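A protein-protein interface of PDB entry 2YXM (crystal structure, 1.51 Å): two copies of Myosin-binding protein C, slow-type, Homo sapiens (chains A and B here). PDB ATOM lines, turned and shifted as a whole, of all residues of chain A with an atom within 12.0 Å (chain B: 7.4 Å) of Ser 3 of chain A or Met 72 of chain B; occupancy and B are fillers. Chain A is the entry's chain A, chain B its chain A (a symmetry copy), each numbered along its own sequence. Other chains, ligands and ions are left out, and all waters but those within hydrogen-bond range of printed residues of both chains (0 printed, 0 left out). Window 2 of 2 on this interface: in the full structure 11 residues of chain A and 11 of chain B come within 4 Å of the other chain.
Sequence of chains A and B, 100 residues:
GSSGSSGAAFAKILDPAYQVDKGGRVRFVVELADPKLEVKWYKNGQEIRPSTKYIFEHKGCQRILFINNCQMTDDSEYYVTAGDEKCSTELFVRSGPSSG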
ATOM      1  N   SER A   3      32.871  11.694  -9.428  1.00  0.00           N
ATOM      2  CA  SER A   3      31.958  10.646  -8.886  1.00  0.00           C
ATOM      3  C   SER A   3      32.080  10.533  -7.375  1.00  0.00           C
ATOM      4  O   SER A   3      33.148  10.763  -6.807  1.00  0.00           O
ATOM      5  CB  SER A   3      32.272   9.287  -9.519  1.00  0.00           C
ATOM      6  OG  SER A   3      31.509   8.254  -8.911  1.00  0.00           O
ATOM      7  N   GLY A   4      30.975  10.174  -6.730  1.00  0.00           N
ATOM      8  CA  GLY A   4      30.981  10.023  -5.289  1.00  0.00           C
ATOM      9  C   GLY A   4      31.842   8.849  -4.864  1.00  0.00           C
ATOM     10  O   GLY A   4      32.140   8.690  -3.683  1.00  0.00           O
ATOM     11  N   SER A   5      32.245   8.025  -5.827  1.00  0.00           N
ATOM     12  CA  SER A   5      33.074   6.858  -5.542  1.00  0.00           C
ATOM     13  C   SER A   5      34.371   7.241  -4.839  1.00  0.00           C
ATOM     14  O   SER A   5      34.805   6.564  -3.909  1.00  0.00           O
ATOM     15  CB  SER A   5      33.403   6.111  -6.838  1.00  0.00           C
ATOM     16  OG  SER A   5      34.309   5.049  -6.596  1.00  0.00           O
ATOM     17  N   SER A   6      34.988   8.331  -5.281  1.00  0.00           N
ATOM     18  CA  SER A   6      36.240   8.774  -4.678  1.00  0.00           C
ATOM     19  C   SER A   6      36.031   9.360  -3.284  1.00  0.00           C
ATOM     20  O   SER A   6      36.989   9.759  -2.619  1.00  0.00           O
ATOM     21  CB  SER A   6      36.926   9.804  -5.582  1.00  0.00           C
ATOM     22  OG  SER A   6      36.122  10.957  -5.755  1.00  0.00           O
ATOM     23  N   GLY A   7      34.778   9.406  -2.841  1.00  0.00           N
ATOM     24  CA  GLY A   7      34.480   9.940  -1.525  1.00  0.00           C
ATOM     25  C   GLY A   7      34.006   8.881  -0.545  1.00  0.00           C
ATOM     26  O   GLY A   7      33.641   9.197   0.587  1.00  0.00           O
ATOM     27  N   ALA A   8      34.010   7.621  -0.973  1.00  0.00           N
ATOM     28  CA  ALA A   8      33.563   6.528  -0.110  1.00  0.00           C
ATOM     29  C   ALA A   8      34.365   6.527   1.184  1.00  0.00           C
ATOM     30  O   ALA A   8      35.596   6.498   1.160  1.00  0.00           O
ATOM     31  CB  ALA A   8      33.722   5.197  -0.829  1.00  0.00           C
ATOM     32  N   ALA A   9      33.663   6.542   2.312  1.00  0.00           N
ATOM     33  CA  ALA A   9      34.321   6.579   3.613  1.00  0.00           C
ATOM     34  C   ALA A   9      33.927   5.462   4.575  1.00  0.00           C
ATOM     35  O   ALA A   9      34.625   5.217   5.557  1.00  0.00           O
ATOM     36  CB  ALA A   9      34.055   7.927   4.273  1.00  0.00           C
ATOM     37  N   GLY A  83      33.470  12.054   6.492  1.00  0.00           N
ATOM     38  CA  GLY A  83      33.847  12.623   5.213  1.00  0.00           C
ATOM     39  C   GLY A  83      32.636  13.328   4.634  1.00  0.00           C
ATOM     40  O   GLY A  83      31.986  14.113   5.324  1.00  0.00           O
ATOM     41  N   ASP A  84      32.312  13.046   3.377  1.00  0.00           N
ATOM     42  CA  ASP A  84      31.162  13.670   2.744  1.00  0.00           C
ATOM     43  C   ASP A  84      29.958  12.733   2.727  1.00  0.00           C
ATOM     44  O   ASP A  84      28.978  12.990   2.033  1.00  0.00           O
ATOM     45  CB  ASP A  84      31.505  14.091   1.310  1.00  0.00           C
ATOM     46  CG  ASP A  84      32.612  15.127   1.255  1.00  0.00           C
ATOM     47  OD1 ASP A  84      33.763  14.795   1.613  1.00  0.00           O
ATOM     48  OD2 ASP A  84      32.328  16.277   0.858  1.00  0.00           O
ATOM     49  N   GLU A  85      30.027  11.654   3.503  1.00  0.00           N
ATOM     50  CA  GLU A  85      28.929  10.695   3.544  1.00  0.00           C
ATOM     51  C   GLU A  85      28.258  10.583   4.906  1.00  0.00           C
ATOM     52  O   GLU A  85      28.748  11.094   5.912  1.00  0.00           O
ATOM     53  CB  GLU A  85      29.418   9.304   3.128  1.00  0.00           C
ATOM     54  CG  GLU A  85      30.071   9.253   1.757  1.00  0.00           C
ATOM     55  CD  GLU A  85      30.433   7.842   1.355  1.00  0.00           C
ATOM     56  OE1 GLU A  85      30.853   7.067   2.238  1.00  0.00           O
ATOM     57  OE2 GLU A  85      30.307   7.510   0.156  1.00  0.00           O
ATOM     58  N   VAL B  20      27.308   2.037 -11.632  1.00  0.00           N
ATOM     59  CA  VAL B  20      26.815   1.830 -12.985  1.00  0.00           C
ATOM     60  C   VAL B  20      27.775   2.504 -13.956  1.00  0.00           C
ATOM     61  O   VAL B  20      28.406   3.509 -13.623  1.00  0.00           O
ATOM     62  CB  VAL B  20      25.390   2.433 -13.150  1.00  0.00           C
ATOM     63  CG1 VAL B  20      25.438   3.940 -12.961  1.00  0.00           C
ATOM     64  CG2 VAL B  20      24.812   2.074 -14.512  1.00  0.00           C
ATOM     65  N   LYS B  22      28.720   4.600 -17.393  1.00  0.00           N
ATOM     66  CA  LYS B  22      28.084   5.694 -18.117  1.00  0.00           C
ATOM     67  C   LYS B  22      27.255   5.121 -19.259  1.00  0.00           C
ATOM     68  O   LYS B  22      27.718   4.244 -19.994  1.00  0.00           O
ATOM     69  CB  LYS B  22      29.132   6.654 -18.682  1.00  0.00           C
ATOM     70  CG  LYS B  22      29.859   7.475 -17.634  1.00  0.00           C
ATOM     71  CD  LYS B  22      30.818   8.460 -18.284  1.00  0.00           C
ATOM     72  CE  LYS B  22      31.500   9.336 -17.246  1.00  0.00           C
ATOM     73  NZ  LYS B  22      32.459  10.285 -17.878  1.00  0.00           N
ATOM     74  N   GLY B  23      26.031   5.622 -19.397  1.00  0.00           N
ATOM     75  CA  GLY B  23      25.142   5.153 -20.445  1.00  0.00           C
ATOM     76  C   GLY B  23      24.396   3.894 -20.047  1.00  0.00           C
ATOM     77  O   GLY B  23      23.504   3.434 -20.764  1.00  0.00           O
ATOM     78  N   LYS B  43      15.695  12.253  -5.358  1.00  0.00           N
ATOM     79  CA  LYS B  43      17.073  12.402  -5.784  1.00  0.00           C
ATOM     80  C   LYS B  43      17.579  13.626  -5.046  1.00  0.00           C
ATOM     81  O   LYS B  43      17.102  14.737  -5.273  1.00  0.00           O
ATOM     82  CB  LYS B  43      17.179  12.634  -7.290  1.00  0.00           C
ATOM     83  CG  LYS B  43      18.612  12.885  -7.745  1.00  0.00           C
ATOM     84  CD  LYS B  43      18.681  13.260  -9.209  1.00  0.00           C
ATOM     85  CE  LYS B  43      20.109  13.542  -9.631  1.00  0.00           C
ATOM     86  NZ  LYS B  43      20.170  13.968 -11.052  1.00  0.00           N
ATOM     87  N   ASN B  69      20.222   5.362 -18.975  1.00  0.00           N
ATOM     88  CA  ASN B  69      21.271   6.208 -19.539  1.00  0.00           C
ATOM     89  C   ASN B  69      21.968   7.028 -18.464  1.00  0.00           C
ATOM     90  O   ASN B  69      22.005   8.257 -18.520  1.00  0.00           O
ATOM     91  CB  ASN B  69      20.669   7.130 -20.602  1.00  0.00           C
ATOM     92  CG  ASN B  69      21.715   7.971 -21.303  1.00  0.00           C
ATOM     93  OD1 ASN B  69      22.867   7.558 -21.447  1.00  0.00           O
ATOM     94  ND2 ASN B  69      21.312   9.149 -21.763  1.00  0.00           N
ATOM     95  N   CYS B  70      22.542   6.332 -17.491  1.00  0.00           N
ATOM     96  CA  CYS B  70      23.210   6.997 -16.384  1.00  0.00           C
ATOM     97  C   CYS B  70      24.439   7.800 -16.777  1.00  0.00           C
ATOM     98  O   CYS B  70      25.309   7.331 -17.509  1.00  0.00           O
ATOM     99  CB  CYS B  70      23.575   5.973 -15.305  1.00  0.00           C
ATOM    100  SG  CYS B  70      22.129   5.319 -14.433  1.00  0.00           S
ATOM    101  N   GLN B  71      24.487   9.028 -16.278  1.00  0.00           N
ATOM    102  CA  GLN B  71      25.597   9.931 -16.535  1.00  0.00           C
ATOM    103  C   GLN B  71      26.026  10.501 -15.189  1.00  0.00           C
ATOM    104  O   GLN B  71      25.407  10.207 -14.167  1.00  0.00           O
ATOM    105  CB  GLN B  71      25.159  11.056 -17.477  1.00  0.00           C
ATOM    106  CG  GLN B  71      24.679  10.591 -18.854  1.00  0.00           C
ATOM    107  CD  GLN B  71      25.732   9.808 -19.620  1.00  0.00           C
ATOM    108  OE1 GLN B  71      26.921  10.130 -19.572  1.00  0.00           O
ATOM    109  NE2 GLN B  71      25.298   8.783 -20.346  1.00  0.00           N
ATOM    110  N   MET B  72      27.075  11.315 -15.177  1.00  0.00           N
ATOM    111  CA  MET B  72      27.552  11.886 -13.926  1.00  0.00           C
ATOM    112  C   MET B  72      26.473  12.707 -13.225  1.00  0.00           C
ATOM    113  O   MET B  72      26.517  12.894 -12.010  1.00  0.00           O
ATOM    114  CB  MET B  72      28.803  12.735 -14.169  1.00  0.00           C
ATOM    115  CG  MET B  72      29.982  11.947 -14.745  1.00  0.00           C
ATOM    116  SD  MET B  72      30.321  10.355 -13.930  1.00  0.00           S
ATOM    117  CE  MET B  72      30.468  10.862 -12.235  1.00  0.00           C
ATOM    118  N   THR B  73      25.500  13.189 -13.992  1.00  0.00           N
ATOM    119  CA  THR B  73      24.403  13.964 -13.426  1.00  0.00           C
ATOM    120  C   THR B  73      23.562  13.075 -12.503  1.00  0.00           C
ATOM    121  O   THR B  73      22.865  13.570 -11.614  1.00  0.00           O
ATOM    122  CB  THR B  73      23.503  14.538 -14.540  1.00  0.00           C
ATOM    123  OG1 THR B  73      23.116  13.488 -15.433  1.00  0.00           O
ATOM    124  CG2 THR B  73      24.250  15.602 -15.327  1.00  0.00           C
ATOM    125  N   ASP B  74      23.644  11.765 -12.712  1.00  0.00           N
ATOM    126  CA  ASP B  74      22.893  10.804 -11.906  1.00  0.00           C
ATOM    127  C   ASP B  74      23.678  10.339 -10.686  1.00  0.00           C
ATOM    128  O   ASP B  74      23.133   9.673  -9.807  1.00  0.00           O
ATOM    129  CB  ASP B  74      22.507   9.589 -12.752  1.00  0.00           C
ATOM    130  CG  ASP B  74      21.638   9.959 -13.931  1.00  0.00           C
ATOM    131  OD1 ASP B  74      20.522  10.475 -13.711  1.00  0.00           O
ATOM    132  OD2 ASP B  74      22.075   9.732 -15.079  1.00  0.00           O
ATOM    133  N   ASP B  75      24.963  10.676 -10.643  1.00  0.00           N
ATOM    134  CA  ASP B  75      25.813  10.308  -9.513  1.00  0.00           C
ATOM    135  C   ASP B  75      25.319  11.163  -8.349  1.00  0.00           C
ATOM    136  O   ASP B  75      25.571  12.367  -8.295  1.00  0.00           O
ATOM    137  CB  ASP B  75      27.274  10.619  -9.848  1.00  0.00           C
ATOM    138  CG  ASP B  75      28.240  10.089  -8.809  1.00  0.00           C
ATOM    139  OD1 ASP B  75      28.258  10.635  -7.686  1.00  0.00           O
ATOM    140  OD2 ASP B  75      28.976   9.126  -9.118  1.00  0.00           O
ATOM    141  N   SER B  76      24.624  10.533  -7.407  1.00  0.00           N
ATOM    142  CA  SER B  76      24.038  11.278  -6.308  1.00  0.00           C
ATOM    143  C   SER B  76      23.475  10.358  -5.237  1.00  0.00           C
ATOM    144  O   SER B  76      23.523   9.133  -5.357  1.00  0.00           O
ATOM    145  CB  SER B  76      22.912  12.150  -6.881  1.00  0.00           C
ATOM    146  OG  SER B  76      22.055  12.674  -5.885  1.00  0.00           O
ATOM    147  N   TYR B  78      20.206   9.037  -3.134  1.00  0.00           N
ATOM    148  CA  TYR B  78      18.794   8.822  -3.430  1.00  0.00           C
ATOM    149  C   TYR B  78      18.141   8.213  -2.212  1.00  0.00           C
ATOM    150  O   TYR B  78      18.797   7.551  -1.415  1.00  0.00           O
ATOM    151  CB  TYR B  78      18.615   7.810  -4.568  1.00  0.00           C
ATOM    152  CG  TYR B  78      19.092   8.269  -5.915  1.00  0.00           C
ATOM    153  CD1 TYR B  78      18.209   8.839  -6.827  1.00  0.00           C
ATOM    154  CD2 TYR B  78      20.434   8.158  -6.271  1.00  0.00           C
ATOM    155  CE1 TYR B  78      18.651   9.295  -8.062  1.00  0.00           C
ATOM    156  CE2 TYR B  78      20.889   8.609  -7.501  1.00  0.00           C
ATOM    157  CZ  TYR B  78      19.994   9.179  -8.390  1.00  0.00           C
ATOM    158  OH  TYR B  78      20.445   9.647  -9.600  1.00  0.00           O
ATOM    159  N   LEU B  91      24.595   6.421  -5.491  1.00  0.00           N
ATOM    160  CA  LEU B  91      24.817   5.861  -6.818  1.00  0.00           C
ATOM    161  C   LEU B  91      26.126   6.413  -7.357  1.00  0.00           C
ATOM    162  O   LEU B  91      26.296   7.629  -7.456  1.00  0.00           O
ATOM    163  CB  LEU B  91      23.687   6.242  -7.782  1.00  0.00           C
ATOM    164  CG  LEU B  91      23.916   5.764  -9.222  1.00  0.00           C
ATOM    165  CD1 LEU B  91      23.949   4.239  -9.262  1.00  0.00           C
ATOM    166  CD2 LEU B  91      22.809   6.297 -10.122  1.00  0.00           C
ATOM    167  N   PHE B  92      27.048   5.517  -7.696  1.00  0.00           N
ATOM    168  CA  PHE B  92      28.336   5.920  -8.248  1.00  0.00           C
ATOM    169  C   PHE B  92      28.351   5.612  -9.739  1.00  0.00           C
ATOM    170  O   PHE B  92      28.207   4.461 -10.140  1.00  0.00           O
ATOM    171  CB  PHE B  92      29.487   5.166  -7.574  1.00  0.00           C
ATOM    172  CG  PHE B  92      29.584   5.383  -6.090  1.00  0.00           C
ATOM    173  CD1 PHE B  92      29.155   6.575  -5.511  1.00  0.00           C
ATOM    174  CD2 PHE B  92      30.146   4.408  -5.273  1.00  0.00           C
ATOM    175  CE1 PHE B  92      29.284   6.792  -4.137  1.00  0.00           C
ATOM    176  CE2 PHE B  92      30.282   4.613  -3.898  1.00  0.00           C
ATOM    177  CZ  PHE B  92      29.850   5.808  -3.327  1.00  0.00           C
ATOM    178  N   VAL B  93      28.525   6.646 -10.553  1.00  0.00           N
ATOM    179  CA  VAL B  93      28.568   6.474 -11.997  1.00  0.00           C
ATOM    180  C   VAL B  93      30.025   6.466 -12.438  1.00  0.00           C
ATOM    181  O   VAL B  93      30.780   7.386 -12.123  1.00  0.00           O
ATOM    182  CB  VAL B  93      27.822   7.618 -12.719  1.00  0.00           C
ATOM    183  CG1 VAL B  93      27.841   7.384 -14.224  1.00  0.00           C
ATOM    184  CG2 VAL B  93      26.388   7.700 -12.218  1.00  0.00           C
ATOM    185  N   ARG B  94      30.418   5.417 -13.152  1.00  0.00           N
ATOM    186  CA  ARG B  94      31.790   5.298 -13.633  1.00  0.00           C
ATOM    187  C   ARG B  94      31.936   5.942 -15.006  1.00  0.00           C
ATOM    188  O   ARG B  94      31.825   5.210 -16.014  1.00  0.00           O
ATOM    189  CB  ARG B  94      32.210   3.832 -13.710  1.00  0.00           C
ATOM    190  CG  ARG B  94      33.659   3.655 -14.131  1.00  0.00           C
ATOM    191  CD  ARG B  94      34.060   2.198 -14.178  1.00  0.00           C
ATOM    192  NE  ARG B  94      35.482   2.028 -14.472  1.00  0.00           N
ATOM    193  CZ  ARG B  94      36.468   2.519 -13.725  1.00  0.00           C
ATOM    194  NH1 ARG B  94      36.197   3.219 -12.631  1.00  0.00           N
ATOM    195  NH2 ARG B  94      37.730   2.307 -14.074  1.00  0.00           N
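OG of Ser 3 of chain A is in hydrogen-bond range of OD2 of Asp 75 of chain B, at 2.7 Å. The side-chain hydroxyl (OG) of Ser 3 of chain A is in hydrogen-bond range of the backbone carbonyl oxygen (O) of Val 93 of chain B (3.4 Å). The backbone NH of Gly 4 of chain A is in hydrogen-bond range of the side-chain carboxylate of Asp 75 of chain B.
The side-chain hydroxyl (OG) of Ser 3 of chain A lies close to the backbone NH (N) of Ser 5 of chain A. OG of Ser 6 of chain A is in hydrogen-bond range of O of Ser 3 of chain A, 3.2 Å away. N of Ala 9 of chain A lies within hydrogen-bond range of OE1 of Glu 85 of chain A, 2.9 Å away. O of Phe 92 of chain B is in hydrogen-bond range of N of Val 20 of chain B (3.0 Å). The backbone NH of Val 93 of chain B sits at hydrogen-bond distance from the side-chain carboxylate of Asp 75 of chain B (2.9 Å).
Among the printed residues, pairs that only touch across the chains: Ser 3 of chain A with Met 72 of chain B (3.6 Å), Ser 3 of chain A with Phe 92 of chain B (3.9 Å), Gly 4 of chain A with Phe 92 of chain B (3.4 Å), Ser 5 of chain A with Phe 92 of chain B (3.4 Å) and Glu 85 of chain A with Phe 92 of chain B (3.9 Å).
Printed residues of chain B within 4 Å of Gly 4 of chain A: Asp 75 (2.9 Å) and Phe 92 (3.4 Å). Of the printed residues of chain B, Ser 5 of chain A touches Phe 92 (3.4 Å). Of the printed residues of chain B, Glu 85 of chain A touches Phe 92 (3.9 Å). No residue of chain A comes within 4 Å of Gln 71 of chain B. Of chain A, only Ser 3 comes within 4 Å of Met 72 of chain B. Asp 74 of chain B touches none of the printed residues of chain A. Asp 75 of chain B touches just these residues of chain A: Ser 3 (2.7 Å) and Gly 4 (2.9 Å). Phe 92 of chain B touches just these residues of chain A: Ser 3, Gly 4, Ser 5 and Glu 85. Of chain A, only Ser 3 (3.4 Å) comes within 4 Å of Val 93 of chain B. The nearest residue of chain B that does not touch Ser 3 of chain A is Arg 94 of chain B (5.2 Å). The nearest residue of chain A that does not touch Met 72 of chain B is Gly 4 of chain A (5.6 Å). The nearest printed residue of chain B that does not touch Ser 5 of chain A is Asp 75 of chain B (4.8 Å).
Of the 10 printed residues of chain A, 4 touch a printed residue of chain B. Of the 17 printed residues of chain B, 4 touch a printed residue of chain A. Hydrophobic or aromatic side chains of chain B within 4 Å of the printed part of chain A: Met 72 and Phe 92. Among the printed residues, 8 pairs touch across the chains. Among the printed residues, no Asp or Glu carboxylate lies within 4 Å of a Lys or Arg side-chain nitrogen of the other chain.
No position is printed for both chains. Of the 8 pairs that touch across the chains among the printed residues, none has its exchanged pair printed and touching as well.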
